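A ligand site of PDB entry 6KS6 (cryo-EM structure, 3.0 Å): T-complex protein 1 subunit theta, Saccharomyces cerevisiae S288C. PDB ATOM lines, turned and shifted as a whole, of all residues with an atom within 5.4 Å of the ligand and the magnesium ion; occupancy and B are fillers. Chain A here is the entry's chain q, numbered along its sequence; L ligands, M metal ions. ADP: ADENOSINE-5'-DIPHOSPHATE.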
ATOM      1  N   MET A  46      29.406 -18.856  36.967  1.00  0.00           N
ATOM      2  CA  MET A  46      29.015 -17.857  35.974  1.00  0.00           C
ATOM      3  C   MET A  46      30.003 -17.824  34.811  1.00  0.00           C
ATOM      4  O   MET A  46      31.214 -17.855  35.017  1.00  0.00           O
ATOM      5  CB  MET A  46      28.914 -16.474  36.625  1.00  0.00           C
ATOM      6  CG  MET A  46      28.533 -15.359  35.679  1.00  0.00           C
ATOM      7  SD  MET A  46      26.848 -15.517  35.048  1.00  0.00           S
ATOM      8  CE  MET A  46      26.739 -14.079  33.981  1.00  0.00           C
ATOM      9  N   GLY A  47      29.471 -17.749  33.598  1.00  0.00           N
ATOM     10  CA  GLY A  47      30.278 -17.635  32.411  1.00  0.00           C
ATOM     11  C   GLY A  47      30.566 -18.980  31.760  1.00  0.00           C
ATOM     12  O   GLY A  47      30.196 -20.035  32.283  1.00  0.00           O
ATOM     13  N   PRO A  48      31.231 -18.954  30.597  1.00  0.00           N
ATOM     14  CA  PRO A  48      31.589 -20.214  29.953  1.00  0.00           C
ATOM     15  C   PRO A  48      32.635 -21.007  30.711  1.00  0.00           C
ATOM     16  O   PRO A  48      32.701 -22.227  30.564  1.00  0.00           O
ATOM     17  CB  PRO A  48      32.112 -19.760  28.572  1.00  0.00           C
ATOM     18  CG  PRO A  48      32.624 -18.386  28.827  1.00  0.00           C
ATOM     19  CD  PRO A  48      31.698 -17.783  29.841  1.00  0.00           C
ATOM     20  N   ASP A  98      15.917 -17.705  30.697  1.00  0.00           N
ATOM     21  CA  ASP A  98      17.295 -17.304  30.451  1.00  0.00           C
ATOM     22  C   ASP A  98      17.658 -16.182  31.412  1.00  0.00           C
ATOM     23  O   ASP A  98      16.844 -15.284  31.659  1.00  0.00           O
ATOM     24  CB  ASP A  98      17.484 -16.856  28.993  1.00  0.00           C
ATOM     25  CG  ASP A  98      18.940 -16.573  28.654  1.00  0.00           C
ATOM     26  OD1 ASP A  98      19.823 -16.813  29.504  1.00  0.00           O
ATOM     27  OD2 ASP A  98      19.201 -16.108  27.526  1.00  0.00           O
ATOM     28  N   GLY A  99      18.883 -16.225  31.928  1.00  0.00           N
ATOM     29  CA  GLY A  99      19.346 -15.216  32.858  1.00  0.00           C
ATOM     30  C   GLY A  99      19.215 -15.563  34.317  1.00  0.00           C
ATOM     31  O   GLY A  99      19.238 -14.645  35.158  1.00  0.00           O
ATOM     32  N   THR A 100      19.059 -16.846  34.666  1.00  0.00           N
ATOM     33  CA  THR A 100      18.904 -17.218  36.069  1.00  0.00           C
ATOM     34  C   THR A 100      20.158 -16.921  36.873  1.00  0.00           C
ATOM     35  O   THR A 100      20.070 -16.537  38.046  1.00  0.00           O
ATOM     36  CB  THR A 100      18.536 -18.703  36.179  1.00  0.00           C
ATOM     37  OG1 THR A 100      19.571 -19.492  35.585  1.00  0.00           O
ATOM     38  CG2 THR A 100      17.220 -18.982  35.463  1.00  0.00           C
ATOM     39  N   ASN A 101      21.336 -17.078  36.268  1.00  0.00           N
ATOM     40  CA  ASN A 101      22.575 -16.791  36.973  1.00  0.00           C
ATOM     41  C   ASN A 101      22.756 -15.288  37.184  1.00  0.00           C
ATOM     42  O   ASN A 101      23.387 -14.879  38.162  1.00  0.00           O
ATOM     43  CB  ASN A 101      23.768 -17.366  36.217  1.00  0.00           C
ATOM     44  CG  ASN A 101      23.809 -18.887  36.265  1.00  0.00           C
ATOM     45  OD1 ASN A 101      23.245 -19.498  37.174  1.00  0.00           O
ATOM     46  ND2 ASN A 101      24.477 -19.489  35.298  1.00  0.00           N
ATOM     47  N   LEU A 102      22.231 -14.471  36.275  1.00  0.00           N
ATOM     48  CA  LEU A 102      22.397 -13.021  36.414  1.00  0.00           C
ATOM     49  C   LEU A 102      21.534 -12.467  37.536  1.00  0.00           C
ATOM     50  O   LEU A 102      21.938 -11.528  38.226  1.00  0.00           O
ATOM     51  CB  LEU A 102      22.055 -12.336  35.088  1.00  0.00           C
ATOM     52  CG  LEU A 102      22.116 -10.806  35.079  1.00  0.00           C
ATOM     53  CD1 LEU A 102      23.533 -10.326  35.358  1.00  0.00           C
ATOM     54  CD2 LEU A 102      21.610 -10.256  33.755  1.00  0.00           C
ATOM     55  N   PRO A 165      25.258 -17.833  21.363  1.00  0.00           N
ATOM     56  CA  PRO A 165      25.834 -17.201  22.557  1.00  0.00           C
ATOM     57  C   PRO A 165      25.323 -17.795  23.862  1.00  0.00           C
ATOM     58  O   PRO A 165      26.070 -17.823  24.854  1.00  0.00           O
ATOM     59  CB  PRO A 165      25.436 -15.734  22.411  1.00  0.00           C
ATOM     60  CG  PRO A 165      25.295 -15.535  20.952  1.00  0.00           C
ATOM     61  CD  PRO A 165      24.685 -16.812  20.464  1.00  0.00           C
ATOM     62  N   VAL A 166      24.069 -18.261  23.894  1.00  0.00           N
ATOM     63  CA  VAL A 166      23.555 -18.904  25.098  1.00  0.00           C
ATOM     64  C   VAL A 166      24.235 -20.244  25.314  1.00  0.00           C
ATOM     65  O   VAL A 166      24.573 -20.607  26.454  1.00  0.00           O
ATOM     66  CB  VAL A 166      22.030 -19.039  25.014  1.00  0.00           C
ATOM     67  CG1 VAL A 166      21.485 -19.796  26.221  1.00  0.00           C
ATOM     68  CG2 VAL A 166      21.376 -17.675  24.896  1.00  0.00           C
ATOM     69  N   SER A 168      27.183 -20.953  24.346  1.00  0.00           N
ATOM     70  CA  SER A 168      28.596 -20.726  24.623  1.00  0.00           C
ATOM     71  C   SER A 168      28.894 -20.805  26.122  1.00  0.00           C
ATOM     72  O   SER A 168      29.982 -21.251  26.510  1.00  0.00           O
ATOM     73  CB  SER A 168      29.036 -19.375  24.066  1.00  0.00           C
ATOM     74  OG  SER A 168      28.353 -18.310  24.703  1.00  0.00           O
ATOM     75  N   SER A 169      27.954 -20.386  26.967  1.00  0.00           N
ATOM     76  CA  SER A 169      28.184 -20.399  28.401  1.00  0.00           C
ATOM     77  C   SER A 169      28.088 -21.802  28.984  1.00  0.00           C
ATOM     78  O   SER A 169      28.971 -22.246  29.727  1.00  0.00           O
ATOM     79  CB  SER A 169      27.195 -19.464  29.098  1.00  0.00           C
ATOM     80  OG  SER A 169      25.862 -19.891  28.909  1.00  0.00           O
ATOM     81  N   LYS A 170      27.015 -22.529  28.665  1.00  0.00           N
ATOM     82  CA  LYS A 170      26.791 -23.863  29.185  1.00  0.00           C
ATOM     83  C   LYS A 170      27.394 -24.895  28.241  1.00  0.00           C
ATOM     84  O   LYS A 170      27.067 -24.925  27.050  1.00  0.00           O
ATOM     85  CB  LYS A 170      25.298 -24.140  29.384  1.00  0.00           C
ATOM     86  CG  LYS A 170      24.742 -23.712  30.736  1.00  0.00           C
ATOM     87  CD  LYS A 170      24.717 -22.196  30.893  1.00  0.00           C
ATOM     88  CE  LYS A 170      24.154 -21.792  32.244  1.00  0.00           C
ATOM     89  NZ  LYS A 170      24.124 -20.309  32.400  1.00  0.00           N
ATOM     90  N   TYR A 172      30.659 -25.192  27.316  1.00  0.00           N
ATOM     91  CA  TYR A 172      31.497 -24.442  26.378  1.00  0.00           C
ATOM     92  C   TYR A 172      32.352 -25.347  25.504  1.00  0.00           C
ATOM     93  O   TYR A 172      32.799 -24.901  24.438  1.00  0.00           O
ATOM     94  CB  TYR A 172      32.390 -23.470  27.167  1.00  0.00           C
ATOM     95  CG  TYR A 172      33.381 -22.699  26.329  1.00  0.00           C
ATOM     96  CD1 TYR A 172      32.977 -21.611  25.573  1.00  0.00           C
ATOM     97  CD2 TYR A 172      34.722 -23.055  26.297  1.00  0.00           C
ATOM     98  CE1 TYR A 172      33.875 -20.892  24.801  1.00  0.00           C
ATOM     99  CE2 TYR A 172      35.633 -22.353  25.531  1.00  0.00           C
ATOM    100  CZ  TYR A 172      35.203 -21.275  24.790  1.00  0.00           C
ATOM    101  OH  TYR A 172      36.110 -20.564  24.025  1.00  0.00           O
ATOM    102  N   GLU A 175      30.356 -26.055  20.660  1.00  0.00           N
ATOM    103  CA  GLU A 175      29.772 -24.815  20.138  1.00  0.00           C
ATOM    104  C   GLU A 175      28.958 -25.099  18.875  1.00  0.00           C
ATOM    105  O   GLU A 175      27.728 -24.981  18.915  1.00  0.00           O
ATOM    106  CB  GLU A 175      30.872 -23.788  19.879  1.00  0.00           C
ATOM    107  CG  GLU A 175      31.573 -23.287  21.126  1.00  0.00           C
ATOM    108  CD  GLU A 175      32.688 -22.315  20.821  1.00  0.00           C
ATOM    109  OE1 GLU A 175      33.036 -22.156  19.629  1.00  0.00           O
ATOM    110  OE2 GLU A 175      33.216 -21.696  21.763  1.00  0.00           O
ATOM    111  N   ASP A 403      17.218 -24.125  27.621  1.00  0.00           N
ATOM    112  CA  ASP A 403      17.490 -22.691  27.683  1.00  0.00           C
ATOM    113  C   ASP A 403      17.703 -22.102  26.293  1.00  0.00           C
ATOM    114  O   ASP A 403      17.476 -20.904  26.101  1.00  0.00           O
ATOM    115  CB  ASP A 403      18.703 -22.421  28.566  1.00  0.00           C
ATOM    116  CG  ASP A 403      18.433 -22.676  30.042  1.00  0.00           C
ATOM    117  OD1 ASP A 403      17.248 -22.760  30.412  1.00  0.00           O
ATOM    118  OD2 ASP A 403      19.406 -22.789  30.808  1.00  0.00           O
ATOM    119  N   GLY A 422      27.629  -8.458  24.524  1.00  0.00           N
ATOM    120  CA  GLY A 422      27.952  -9.296  25.647  1.00  0.00           C
ATOM    121  C   GLY A 422      29.414  -9.207  26.058  1.00  0.00           C
ATOM    122  O   GLY A 422      30.139  -8.300  25.662  1.00  0.00           O
ATOM    123  N   ALA A 423      29.815 -10.184  26.875  1.00  0.00           N
ATOM    124  CA  ALA A 423      31.181 -10.277  27.390  1.00  0.00           C
ATOM    125  C   ALA A 423      31.583  -9.017  28.155  1.00  0.00           C
ATOM    126  O   ALA A 423      32.639  -8.435  27.945  1.00  0.00           O
ATOM    127  CB  ALA A 423      32.179 -10.579  26.263  1.00  0.00           C
ATOM    128  N   GLY A 424      30.695  -8.596  29.061  1.00  0.00           N
ATOM    129  CA  GLY A 424      30.966  -7.431  29.886  1.00  0.00           C
ATOM    130  C   GLY A 424      30.888  -6.098  29.182  1.00  0.00           C
ATOM    131  O   GLY A 424      31.334  -5.096  29.737  1.00  0.00           O
ATOM    132  N   LEU A 463      34.021 -13.089  34.423  1.00  0.00           N
ATOM    133  CA  LEU A 463      34.629 -13.688  33.239  1.00  0.00           C
ATOM    134  C   LEU A 463      36.143 -13.639  33.314  1.00  0.00           C
ATOM    135  O   LEU A 463      36.823 -14.557  32.845  1.00  0.00           O
ATOM    136  CB  LEU A 463      34.134 -12.980  31.978  1.00  0.00           C
ATOM    137  CG  LEU A 463      32.644 -13.084  31.688  1.00  0.00           C
ATOM    138  CD1 LEU A 463      32.267 -12.248  30.475  1.00  0.00           C
ATOM    139  CD2 LEU A 463      32.226 -14.536  31.489  1.00  0.00           C
ATOM    140  N   VAL A 499      35.233  -8.054  27.706  1.00  0.00           N
ATOM    141  CA  VAL A 499      36.194  -8.863  28.454  1.00  0.00           C
ATOM    142  C   VAL A 499      36.665 -10.013  27.575  1.00  0.00           C
ATOM    143  O   VAL A 499      35.865 -10.635  26.858  1.00  0.00           O
ATOM    144  CB  VAL A 499      35.562  -9.379  29.760  1.00  0.00           C
ATOM    145  CG1 VAL A 499      36.526 -10.292  30.503  1.00  0.00           C
ATOM    146  CG2 VAL A 499      35.131  -8.217  30.637  1.00  0.00           C
ATOM    147  N   ILE A 501      38.603 -13.707  27.348  1.00  0.00           N
ATOM    148  CA  ILE A 501      39.024 -14.932  28.020  1.00  0.00           C
ATOM    149  C   ILE A 501      39.895 -15.711  27.037  1.00  0.00           C
ATOM    150  O   ILE A 501      39.388 -16.302  26.082  1.00  0.00           O
ATOM    151  CB  ILE A 501      37.835 -15.768  28.496  1.00  0.00           C
ATOM    152  CG1 ILE A 501      37.043 -15.021  29.566  1.00  0.00           C
ATOM    153  CG2 ILE A 501      38.301 -17.128  29.012  1.00  0.00           C
ATOM    154  CD1 ILE A 501      35.724 -15.671  29.920  1.00  0.00           C
ATOM    155  N   ILE A 517      29.023 -12.445  19.976  1.00  0.00           N
ATOM    156  CA  ILE A 517      28.478 -12.838  21.262  1.00  0.00           C
ATOM    157  C   ILE A 517      27.495 -11.762  21.694  1.00  0.00           C
ATOM    158  O   ILE A 517      27.888 -10.640  22.037  1.00  0.00           O
ATOM    159  CB  ILE A 517      29.589 -13.029  22.316  1.00  0.00           C
ATOM    160  CG1 ILE A 517      30.504 -14.191  21.919  1.00  0.00           C
ATOM    161  CG2 ILE A 517      28.980 -13.279  23.687  1.00  0.00           C
ATOM    162  CD1 ILE A 517      31.758 -14.294  22.758  1.00  0.00           C
ATOM    163  N   ASP A 519      23.482 -10.787  23.663  1.00  0.00           N
ATOM    164  CA  ASP A 519      22.474 -11.132  24.652  1.00  0.00           C
ATOM    165  C   ASP A 519      21.147 -10.488  24.283  1.00  0.00           C
ATOM    166  O   ASP A 519      21.114  -9.436  23.623  1.00  0.00           O
ATOM    167  CB  ASP A 519      22.906 -10.702  26.051  1.00  0.00           C
ATOM    168  CG  ASP A 519      24.061 -11.513  26.598  1.00  0.00           C
ATOM    169  OD1 ASP A 519      24.339 -12.603  26.035  1.00  0.00           O
ATOM    170  OD2 ASP A 519      24.697 -11.072  27.577  1.00  0.00           O
ATOM    171  N   THR A 523      15.687 -10.163  27.852  1.00  0.00           N
ATOM    172  CA  THR A 523      16.158 -10.954  28.970  1.00  0.00           C
ATOM    173  C   THR A 523      16.765 -10.076  30.052  1.00  0.00           C
ATOM    174  O   THR A 523      16.516 -10.289  31.245  1.00  0.00           O
ATOM    175  CB  THR A 523      17.177 -11.985  28.488  1.00  0.00           C
ATOM    176  OG1 THR A 523      16.560 -12.863  27.534  1.00  0.00           O
ATOM    177  CG2 THR A 523      17.717 -12.800  29.658  1.00  0.00           C
ATOM    178  N   LYS A 524      17.557  -9.075  29.663  1.00  0.00           N
ATOM    179  CA  LYS A 524      18.182  -8.197  30.652  1.00  0.00           C
ATOM    180  C   LYS A 524      17.161  -7.302  31.334  1.00  0.00           C
ATOM    181  O   LYS A 524      17.329  -6.976  32.522  1.00  0.00           O
ATOM    182  CB  LYS A 524      19.273  -7.350  29.983  1.00  0.00           C
ATOM    183  CG  LYS A 524      20.358  -8.162  29.315  1.00  0.00           C
ATOM    184  CD  LYS A 524      21.089  -9.035  30.319  1.00  0.00           C
ATOM    185  CE  LYS A 524      22.226  -9.800  29.657  1.00  0.00           C
ATOM    186  NZ  LYS A 524      22.947 -10.674  30.626  1.00  0.00           N
HETATM  187  PB  ADP L   1      22.565 -15.694  31.298  1.00  0.00           P
HETATM  188  O1B ADP L   1      21.692 -14.547  30.821  1.00  0.00           O
HETATM  189  O2B ADP L   1      22.554 -15.921  32.792  1.00  0.00           O
HETATM  190  O3B ADP L   1      22.455 -16.944  30.477  1.00  0.00           O
HETATM  191  PA  ADP L   1      25.310 -16.176  31.021  1.00  0.00           P
HETATM  192  O1A ADP L   1      25.458 -16.737  32.410  1.00  0.00           O
HETATM  193  O2A ADP L   1      25.168 -17.104  29.838  1.00  0.00           O
HETATM  194  O3A ADP L   1      24.063 -15.159  31.009  1.00  0.00           O
HETATM  195  O5' ADP L   1      26.537 -15.181  30.726  1.00  0.00           O
HETATM  196  C5' ADP L   1      27.817 -15.685  30.358  1.00  0.00           C
HETATM  197  C4' ADP L   1      28.598 -14.558  29.699  1.00  0.00           C
HETATM  198  O4' ADP L   1      29.865 -15.030  29.234  1.00  0.00           O
HETATM  199  C3' ADP L   1      27.864 -14.001  28.492  1.00  0.00           C
HETATM  200  O3' ADP L   1      27.367 -12.692  28.784  1.00  0.00           O
HETATM  201  C2' ADP L   1      28.882 -13.941  27.379  1.00  0.00           C
HETATM  202  O2' ADP L   1      29.008 -12.597  26.899  1.00  0.00           O
HETATM  203  C1' ADP L   1      30.192 -14.413  27.981  1.00  0.00           C
HETATM  204  N9  ADP L   1      30.853 -15.387  27.079  1.00  0.00           N
HETATM  205  C8  ADP L   1      30.404 -16.612  26.763  1.00  0.00           C
HETATM  206  N7  ADP L   1      31.239 -17.241  25.908  1.00  0.00           N
HETATM  207  C5  ADP L   1      32.270 -16.414  25.673  1.00  0.00           C
HETATM  208  C6  ADP L   1      33.516 -16.456  24.863  1.00  0.00           C
HETATM  209  N6  ADP L   1      33.826 -17.548  24.121  1.00  0.00           N
HETATM  210  N1  ADP L   1      34.318 -15.368  24.896  1.00  0.00           N
HETATM  211  C2  ADP L   1      34.016 -14.283  25.616  1.00  0.00           C
HETATM  212  N3  ADP L   1      32.911 -14.174  26.379  1.00  0.00           N
HETATM  213  C4  ADP L   1      32.009 -15.193  26.446  1.00  0.00           C
HETATM  214 MG    MG M   1      22.687 -18.790  29.434  1.00  0.00          MG
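SD of Met 46 lies close to O1A of the ligand (3.2 Å). An oxygen (O3B) of the ligand lies close to the side-chain carboxylate (OD1) of Asp 98 (2.8 Å). Merely in contact with the ligand: Gly 47 (3.8 Å), Pro 48 (3.4 Å), Asn 101 (3.9 Å), Leu 102 (3.8 Å), Tyr 172 (3.4 Å), Gly 422 (3.5 Å), Leu 463 (3.3 Å) and Ile 517 (3.3 Å). Hydrophobic or aromatic side chains that line the ligand: Met 46, Pro 48, Tyr 172, Ala 423, Leu 463 and Ile 517. The nearest printed residue that does not touch the ligand is Thr 100 (4.1 Å).
The magnesium ion is bound by O3B of the ligand (2.1 Å). The magnesium ion has one donor atom within binding distance.
Merely in contact with the magnesium ion: Ser 169 (3.4 Å), Asp 98 (3.5 Å), Val 166 (3.6 Å) and Lys 170 (3.6 Å). Of the 26 residues printed, 4 come within 4 Å of the magnesium ion.
The side-chain carboxylate of Asp 519 sits at hydrogen-bond distance from an oxygen (O3') of the ligand, at 3.3 Å. An oxygen (O2') of the ligand sits at hydrogen-bond distance from the backbone NH (N) of Ala 423. The side-chain hydroxyl (OG) of Ser 168 lies within hydrogen-bond range of a nitrogen (N7) of the ligand, 3.3 Å away. The side-chain hydroxyl (OG) of Ser 169 sits at hydrogen-bond distance from an oxygen (O2A) of the ligand. The backbone NH (N) of Gly 99 sits close to an oxygen (O1B) of the ligand. An oxygen (O1A) of the ligand is in salt-bridge range of the side-chain amino group (NZ) of Lys 170.
O of Ile 517 is in hydrogen-bond range of N of Gly 422, 3.3 Å away. The backbone carbonyl oxygen (O) of Ala 423 is in hydrogen-bond range of the backbone NH (N) of Val 499. The side-chain amide nitrogen (ND2) of Asn 101 lies close to the side-chain amino group (NZ) of Lys 170 (3.0 Å). The side-chain carboxylate (OD2) of Asp 519 is in salt-bridge range of the side-chain amino group (NZ) of Lys 524 (3.5 Å). O of Val 166 is in hydrogen-bond range of OG of Ser 169 (2.9 Å).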
